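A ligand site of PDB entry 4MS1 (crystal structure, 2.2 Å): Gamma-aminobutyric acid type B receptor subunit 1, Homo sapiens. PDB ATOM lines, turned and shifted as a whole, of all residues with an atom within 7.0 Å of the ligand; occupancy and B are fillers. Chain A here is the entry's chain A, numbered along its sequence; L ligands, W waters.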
ATOM      1  N   GLY A  16       3.946  14.527   1.296  1.00  0.00           N
ATOM      2  CA  GLY A  16       2.796  14.895   0.476  1.00  0.00           C
ATOM      3  C   GLY A  16       2.906  14.412  -0.954  1.00  0.00           C
ATOM      4  O   GLY A  16       3.712  13.520  -1.247  1.00  0.00           O
ATOM      5  N   GLY A  17       2.101  15.003  -1.844  1.00  0.00           N
ATOM      6  CA  GLY A  17       2.053  14.662  -3.270  1.00  0.00           C
ATOM      7  C   GLY A  17       3.364  14.842  -4.021  1.00  0.00           C
ATOM      8  O   GLY A  17       3.690  14.055  -4.911  1.00  0.00           O
ATOM      9  N   TRP A  18       4.116  15.909  -3.700  1.00  0.00           N
ATOM     10  CA  TRP A  18       5.436  16.167  -4.272  1.00  0.00           C
ATOM     11  C   TRP A  18       6.371  16.475  -3.104  1.00  0.00           C
ATOM     12  O   TRP A  18       6.412  17.609  -2.624  1.00  0.00           O
ATOM     13  CB  TRP A  18       5.433  17.282  -5.334  1.00  0.00           C
ATOM     14  CG  TRP A  18       6.806  17.562  -5.892  1.00  0.00           C
ATOM     15  CD1 TRP A  18       7.560  16.712  -6.657  1.00  0.00           C
ATOM     16  CD2 TRP A  18       7.629  18.722  -5.654  1.00  0.00           C
ATOM     17  NE1 TRP A  18       8.785  17.290  -6.927  1.00  0.00           N
ATOM     18  CE2 TRP A  18       8.830  18.538  -6.359  1.00  0.00           C
ATOM     19  CE3 TRP A  18       7.433  19.931  -4.941  1.00  0.00           C
ATOM     20  CZ2 TRP A  18       9.840  19.516  -6.389  1.00  0.00           C
ATOM     21  CZ3 TRP A  18       8.442  20.877  -4.931  1.00  0.00           C
ATOM     22  CH2 TRP A  18       9.637  20.666  -5.647  1.00  0.00           C
ATOM     23  N   CYS A  56       3.427  19.686   1.506  1.00  0.00           N
ATOM     24  CA  CYS A  56       2.802  19.887   0.198  1.00  0.00           C
ATOM     25  C   CYS A  56       1.282  20.133   0.387  1.00  0.00           C
ATOM     26  O   CYS A  56       0.456  19.739  -0.444  1.00  0.00           O
ATOM     27  CB  CYS A  56       3.109  18.705  -0.719  1.00  0.00           C
ATOM     28  SG  CYS A  56       2.909  19.024  -2.486  1.00  0.00           S
ATOM     29  N   GLY A  81       7.363  25.723  -2.489  1.00  0.00           N
ATOM     30  CA  GLY A  81       7.654  24.652  -3.441  1.00  0.00           C
ATOM     31  C   GLY A  81       6.497  24.212  -4.308  1.00  0.00           C
ATOM     32  O   GLY A  81       6.472  24.542  -5.494  1.00  0.00           O
ATOM     33  N   CYS A  82       5.530  23.438  -3.730  1.00  0.00           N
ATOM     34  CA  CYS A  82       4.313  22.888  -4.390  1.00  0.00           C
ATOM     35  C   CYS A  82       3.458  24.009  -4.972  1.00  0.00           C
ATOM     36  O   CYS A  82       3.442  25.116  -4.439  1.00  0.00           O
ATOM     37  CB  CYS A  82       3.507  21.998  -3.435  1.00  0.00           C
ATOM     38  SG  CYS A  82       4.331  20.406  -3.068  1.00  0.00           S
ATOM     39  N   SER A  83       2.712  23.705  -6.052  1.00  0.00           N
ATOM     40  CA  SER A  83       1.798  24.632  -6.730  1.00  0.00           C
ATOM     41  C   SER A  83       0.656  25.064  -5.804  1.00  0.00           C
ATOM     42  O   SER A  83       0.295  26.223  -5.810  1.00  0.00           O
ATOM     43  CB  SER A  83       1.188  23.979  -7.969  1.00  0.00           C
ATOM     44  OG  SER A  83       2.056  24.092  -9.070  1.00  0.00           O
ATOM     45  N   SER A  84       0.128  24.139  -5.007  1.00  0.00           N
ATOM     46  CA  SER A  84      -0.971  24.418  -4.083  1.00  0.00           C
ATOM     47  C   SER A  84      -0.530  25.404  -2.989  1.00  0.00           C
ATOM     48  O   SER A  84      -1.270  26.320  -2.633  1.00  0.00           O
ATOM     49  CB  SER A  84      -1.542  23.123  -3.506  1.00  0.00           C
ATOM     50  OG  SER A  84      -0.697  22.549  -2.522  1.00  0.00           O
ATOM     51  N   VAL A  85       0.689  25.210  -2.478  1.00  0.00           N
ATOM     52  CA  VAL A  85       1.289  26.059  -1.462  1.00  0.00           C
ATOM     53  C   VAL A  85       1.634  27.444  -2.102  1.00  0.00           C
ATOM     54  O   VAL A  85       1.344  28.478  -1.500  1.00  0.00           O
ATOM     55  CB  VAL A  85       2.517  25.360  -0.797  1.00  0.00           C
ATOM     56  CG1 VAL A  85       3.305  26.344   0.095  1.00  0.00           C
ATOM     57  CG2 VAL A  85       2.069  24.122  -0.002  1.00  0.00           C
ATOM     58  N   TYR A 103      10.442  27.322  -6.465  1.00  0.00           N
ATOM     59  CA  TYR A 103      11.441  26.422  -7.073  1.00  0.00           C
ATOM     60  C   TYR A 103      10.789  25.137  -7.641  1.00  0.00           C
ATOM     61  O   TYR A 103      11.455  24.390  -8.338  1.00  0.00           O
ATOM     62  CB  TYR A 103      12.568  26.077  -6.067  1.00  0.00           C
ATOM     63  CG  TYR A 103      12.050  25.532  -4.754  1.00  0.00           C
ATOM     64  CD1 TYR A 103      11.749  24.181  -4.615  1.00  0.00           C
ATOM     65  CD2 TYR A 103      11.741  26.383  -3.701  1.00  0.00           C
ATOM     66  CE1 TYR A 103      11.149  23.691  -3.458  1.00  0.00           C
ATOM     67  CE2 TYR A 103      11.129  25.908  -2.537  1.00  0.00           C
ATOM     68  CZ  TYR A 103      10.875  24.561  -2.417  1.00  0.00           C
ATOM     69  OH  TYR A 103      10.315  24.083  -1.274  1.00  0.00           O
ATOM     70  N   GLY A 104       9.514  24.873  -7.316  1.00  0.00           N
ATOM     71  CA  GLY A 104       8.874  23.637  -7.787  1.00  0.00           C
ATOM     72  C   GLY A 104       7.478  23.691  -8.394  1.00  0.00           C
ATOM     73  O   GLY A 104       6.924  22.646  -8.682  1.00  0.00           O
ATOM     74  N   SER A 105       6.904  24.884  -8.592  1.00  0.00           N
ATOM     75  CA  SER A 105       5.531  25.035  -9.100  1.00  0.00           C
ATOM     76  C   SER A 105       5.369  24.926 -10.617  1.00  0.00           C
ATOM     77  O   SER A 105       5.953  25.699 -11.368  1.00  0.00           O
ATOM     78  CB  SER A 105       4.923  26.341  -8.590  1.00  0.00           C
ATOM     79  OG  SER A 105       4.850  26.266  -7.174  1.00  0.00           O
ATOM     80  N   SER A 106       4.548  23.973 -11.049  1.00  0.00           N
ATOM     81  CA  SER A 106       4.311  23.686 -12.480  1.00  0.00           C
ATOM     82  C   SER A 106       2.954  24.178 -12.999  1.00  0.00           C
ATOM     83  O   SER A 106       2.779  24.267 -14.218  1.00  0.00           O
ATOM     84  CB  SER A 106       4.398  22.186 -12.719  1.00  0.00           C
ATOM     85  OG  SER A 106       3.295  21.522 -12.117  1.00  0.00           O
ATOM     86  N   SER A 107       2.005  24.458 -12.081  1.00  0.00           N
ATOM     87  CA  SER A 107       0.641  24.851 -12.414  1.00  0.00           C
ATOM     88  C   SER A 107       0.544  26.033 -13.398  1.00  0.00           C
ATOM     89  O   SER A 107       0.958  27.137 -13.069  1.00  0.00           O
ATOM     90  CB  SER A 107      -0.149  25.146 -11.146  1.00  0.00           C
ATOM     91  OG  SER A 107      -1.498  25.462 -11.428  1.00  0.00           O
ATOM     92  N   LEU A 110      -0.572  29.638 -12.089  1.00  0.00           N
ATOM     93  CA  LEU A 110       0.352  30.523 -11.371  1.00  0.00           C
ATOM     94  C   LEU A 110       0.997  31.573 -12.276  1.00  0.00           C
ATOM     95  O   LEU A 110       1.721  32.423 -11.786  1.00  0.00           O
ATOM     96  CB  LEU A 110       1.403  29.724 -10.581  1.00  0.00           C
ATOM     97  CG  LEU A 110       0.944  29.274  -9.195  1.00  0.00           C
ATOM     98  CD1 LEU A 110       1.723  28.077  -8.732  1.00  0.00           C
ATOM     99  CD2 LEU A 110       0.959  30.441  -8.180  1.00  0.00           C
ATOM    100  N   ARG A 121       8.997  32.070 -10.706  1.00  0.00           N
ATOM    101  CA  ARG A 121       9.288  30.648 -10.529  1.00  0.00           C
ATOM    102  C   ARG A 121      10.409  30.162 -11.463  1.00  0.00           C
ATOM    103  O   ARG A 121      10.353  30.445 -12.664  1.00  0.00           O
ATOM    104  CB  ARG A 121       8.010  29.778 -10.650  1.00  0.00           C
ATOM    105  CG  ARG A 121       7.274  29.864 -11.992  1.00  0.00           C
ATOM    106  CD  ARG A 121       6.119  28.904 -12.021  1.00  0.00           C
ATOM    107  NE  ARG A 121       5.087  29.280 -12.985  1.00  0.00           N
ATOM    108  CZ  ARG A 121       3.943  28.628 -13.146  1.00  0.00           C
ATOM    109  NH1 ARG A 121       3.681  27.536 -12.441  1.00  0.00           N
ATOM    110  NH2 ARG A 121       3.043  29.064 -14.037  1.00  0.00           N
ATOM    111  N   HIS A 123      10.981  26.979 -11.783  1.00  0.00           N
ATOM    112  CA  HIS A 123      10.330  25.806 -12.329  1.00  0.00           C
ATOM    113  C   HIS A 123       9.401  26.335 -13.457  1.00  0.00           C
ATOM    114  O   HIS A 123       8.564  27.181 -13.179  1.00  0.00           O
ATOM    115  CB  HIS A 123       9.484  25.062 -11.287  1.00  0.00           C
ATOM    116  CG  HIS A 123       8.988  23.704 -11.742  1.00  0.00           C
ATOM    117  ND1 HIS A 123       8.207  23.558 -12.877  1.00  0.00           N
ATOM    118  CD2 HIS A 123       9.177  22.483 -11.188  1.00  0.00           C
ATOM    119  CE1 HIS A 123       7.970  22.256 -12.985  1.00  0.00           C
ATOM    120  NE2 HIS A 123       8.518  21.573 -11.982  1.00  0.00           N
ATOM    121  N   VAL A 154      -4.435  21.007 -13.678  1.00  0.00           N
ATOM    122  CA  VAL A 154      -3.192  21.136 -14.439  1.00  0.00           C
ATOM    123  C   VAL A 154      -3.342  20.738 -15.919  1.00  0.00           C
ATOM    124  O   VAL A 154      -2.855  21.458 -16.788  1.00  0.00           O
ATOM    125  CB  VAL A 154      -1.975  20.479 -13.732  1.00  0.00           C
ATOM    126  CG1 VAL A 154      -2.170  18.962 -13.514  1.00  0.00           C
ATOM    127  CG2 VAL A 154      -0.668  20.757 -14.470  1.00  0.00           C
ATOM    128  N   TYR A 203      -1.561  11.131 -15.558  1.00  0.00           N
ATOM    129  CA  TYR A 203      -0.551  10.577 -14.659  1.00  0.00           C
ATOM    130  C   TYR A 203      -0.279   9.107 -15.032  1.00  0.00           C
ATOM    131  O   TYR A 203      -0.987   8.538 -15.865  1.00  0.00           O
ATOM    132  CB  TYR A 203      -0.973  10.722 -13.176  1.00  0.00           C
ATOM    133  CG  TYR A 203      -0.935  12.171 -12.712  1.00  0.00           C
ATOM    134  CD1 TYR A 203       0.269  12.857 -12.615  1.00  0.00           C
ATOM    135  CD2 TYR A 203      -2.102  12.841 -12.355  1.00  0.00           C
ATOM    136  CE1 TYR A 203       0.302  14.199 -12.226  1.00  0.00           C
ATOM    137  CE2 TYR A 203      -2.080  14.160 -11.932  1.00  0.00           C
ATOM    138  CZ  TYR A 203      -0.872  14.843 -11.881  1.00  0.00           C
ATOM    139  OH  TYR A 203      -0.846  16.157 -11.503  1.00  0.00           O
ATOM    140  N   TRP A 231       7.459  12.262 -18.152  1.00  0.00           N
ATOM    141  CA  TRP A 231       7.702  12.263 -16.701  1.00  0.00           C
ATOM    142  C   TRP A 231       7.478  10.881 -16.066  1.00  0.00           C
ATOM    143  O   TRP A 231       7.619  10.753 -14.849  1.00  0.00           O
ATOM    144  CB  TRP A 231       6.818  13.352 -16.009  1.00  0.00           C
ATOM    145  CG  TRP A 231       5.320  13.203 -16.176  1.00  0.00           C
ATOM    146  CD1 TRP A 231       4.640  12.171 -16.759  1.00  0.00           C
ATOM    147  CD2 TRP A 231       4.331  14.126 -15.699  1.00  0.00           C
ATOM    148  NE1 TRP A 231       3.290  12.395 -16.673  1.00  0.00           N
ATOM    149  CE2 TRP A 231       3.063  13.576 -16.015  1.00  0.00           C
ATOM    150  CE3 TRP A 231       4.384  15.357 -15.017  1.00  0.00           C
ATOM    151  CZ2 TRP A 231       1.865  14.224 -15.692  1.00  0.00           C
ATOM    152  CZ3 TRP A 231       3.202  15.998 -14.712  1.00  0.00           C
ATOM    153  CH2 TRP A 231       1.958  15.441 -15.060  1.00  0.00           C
ATOM    154  N   MET A 265      15.671  20.226 -16.778  1.00  0.00           N
ATOM    155  CA  MET A 265      15.937  20.716 -15.421  1.00  0.00           C
ATOM    156  C   MET A 265      17.437  20.705 -15.035  1.00  0.00           C
ATOM    157  O   MET A 265      17.803  21.231 -13.984  1.00  0.00           O
ATOM    158  CB  MET A 265      15.099  19.958 -14.395  1.00  0.00           C
ATOM    159  CG  MET A 265      13.624  20.293 -14.484  1.00  0.00           C
ATOM    160  SD  MET A 265      12.741  19.320 -13.291  1.00  0.00           S
ATOM    161  CE  MET A 265      11.057  19.594 -13.813  1.00  0.00           C
ATOM    162  N   GLN A 301      15.311  15.696  -9.175  1.00  0.00           N
ATOM    163  CA  GLN A 301      15.359  16.244 -10.517  1.00  0.00           C
ATOM    164  C   GLN A 301      15.072  17.728 -10.580  1.00  0.00           C
ATOM    165  O   GLN A 301      15.563  18.402 -11.488  1.00  0.00           O
ATOM    166  CB  GLN A 301      14.513  15.444 -11.505  1.00  0.00           C
ATOM    167  CG  GLN A 301      13.028  15.386 -11.202  1.00  0.00           C
ATOM    168  CD  GLN A 301      12.212  15.007 -12.425  1.00  0.00           C
ATOM    169  OE1 GLN A 301      12.729  14.884 -13.565  1.00  0.00           O
ATOM    170  NE2 GLN A 301      10.910  14.849 -12.239  1.00  0.00           N
ATOM    171  N   GLU A 302      14.316  18.248  -9.581  1.00  0.00           N
ATOM    172  CA  GLU A 302      13.983  19.666  -9.482  1.00  0.00           C
ATOM    173  C   GLU A 302      15.029  20.442  -8.695  1.00  0.00           C
ATOM    174  O   GLU A 302      15.050  21.664  -8.770  1.00  0.00           O
ATOM    175  CB  GLU A 302      12.587  19.874  -8.849  1.00  0.00           C
ATOM    176  CG  GLU A 302      11.432  19.480  -9.754  1.00  0.00           C
ATOM    177  CD  GLU A 302      11.031  18.026  -9.717  1.00  0.00           C
ATOM    178  OE1 GLU A 302      11.476  17.288  -8.809  1.00  0.00           O
ATOM    179  OE2 GLU A 302      10.235  17.626 -10.604  1.00  0.00           O
ATOM    180  N   LEU A 305      16.726  23.652  -9.946  1.00  0.00           N
ATOM    181  CA  LEU A 305      15.831  24.824 -10.030  1.00  0.00           C
ATOM    182  C   LEU A 305      15.836  25.569  -8.713  1.00  0.00           C
ATOM    183  O   LEU A 305      15.728  26.795  -8.693  1.00  0.00           O
ATOM    184  CB  LEU A 305      14.392  24.414 -10.391  1.00  0.00           C
ATOM    185  CG  LEU A 305      14.224  23.475 -11.590  1.00  0.00           C
ATOM    186  CD1 LEU A 305      12.819  22.883 -11.650  1.00  0.00           C
ATOM    187  CD2 LEU A 305      14.626  24.137 -12.886  1.00  0.00           C
HETATM  188  O1  LIG L   1       2.902  21.179  -7.130  1.00  0.00           O
HETATM  189  P1  LIG L   1       3.351  20.640  -8.431  1.00  0.00           P
HETATM  190  C1  LIG L   1       5.034  19.970  -8.213  1.00  0.00           C
HETATM  191  C2  LIG L   1       5.678  19.572  -9.543  1.00  0.00           C
HETATM  192  C3  LIG L   1       7.194  19.364  -9.391  1.00  0.00           C
HETATM  193  N1  LIG L   1       7.792  18.974 -10.669  1.00  0.00           N
HETATM  194  O2  LIG L   1       3.332  21.823  -9.522  1.00  0.00           O
HETATM  195  C4  LIG L   1       2.211  19.337  -9.013  1.00  0.00           C
HETATM  196  C5  LIG L   1       2.283  18.010  -8.240  1.00  0.00           C
HETATM  197  C6  LIG L   1       1.687  18.069  -6.817  1.00  0.00           C
HETATM  198  C7  LIG L   1       0.750  16.908  -6.446  1.00  0.00           C
HETATM  199  C8  LIG L   1       1.145  15.519  -7.000  1.00  0.00           C
HETATM  200  C9  LIG L   1       1.663  15.526  -8.439  1.00  0.00           C
HETATM  201  C10 LIG L   1       1.615  16.912  -9.085  1.00  0.00           C
HETATM  202  O   HOH W   1       0.632  21.192  -5.717  1.00  0.00           O
HETATM  203  O   HOH W   2       6.201  17.411 -12.422  1.00  0.00           O
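Gly 17 touches the ligand. Trp 18 touches the ligand (CE2 to C3, 3.5 Å). CA of Cys 82 touches O1 of the ligand (3.5 Å). O of Gly 104 touches C1 of the ligand, at 3.3 Å. C of Ser 105 touches O2 of the ligand, at 3.9 Å. N of Ser 107 touches O2 of the ligand (3.9 Å). Tyr 203 touches the ligand (OH to C10, 3.5 Å). Of the 24 residues printed, 11 come within 4 Å of the ligand.
Water W1 lies within hydrogen-bond range of an oxygen (O1) of the ligand (2.7 Å), the backbone NH of Ser 84 (3.1 Å) and the backbone NH of Ser 83 (3.3 Å).
N of Ser 106 sits at hydrogen-bond distance from OG of Ser 83. The backbone NH of Trp 18 is in hydrogen-bond range of the side-chain sulfur of Cys 56 (3.6 Å). The backbone NH of Ser 107 is in hydrogen-bond range of the side-chain hydroxyl of Ser 83. A ring nitrogen (ND1) of His 123 is in hydrogen-bond range of the backbone carbonyl oxygen (O) of Ser 105, at 3.5 Å. The backbone carbonyl oxygen (O) of Gly 81 is in hydrogen-bond range of the side-chain hydroxyl (OG) of Ser 105, 2.9 Å away. The guanidinium group (NH1) of Arg 121 is in hydrogen-bond range of the backbone carbonyl oxygen (O) of Ser 107, 2.8 Å away. O of Ser 105 is in hydrogen-bond range of NH1 of Arg 121 (3.1 Å). NE1 of Trp 18 sits at hydrogen-bond distance from OE1 of Glu 302 (3.3 Å).
O1 of the ligand lies within hydrogen-bond range of N of Ser 83, 2.8 Å away. N of Ser 106 lies within hydrogen-bond range of O2 of the ligand. OG of Ser 83 is in hydrogen-bond range of O2 of the ligand, at 2.6 Å. A ring nitrogen (NE2) of His 123 sits at hydrogen-bond distance from a nitrogen (N1) of the ligand (3.0 Å). The side-chain hydroxyl of Ser 106 is in hydrogen-bond range of an oxygen (O2) of the ligand. The side-chain carboxylate (OE2) of Glu 302 is in salt-bridge range of a nitrogen (N1) of the ligand (2.8 Å).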
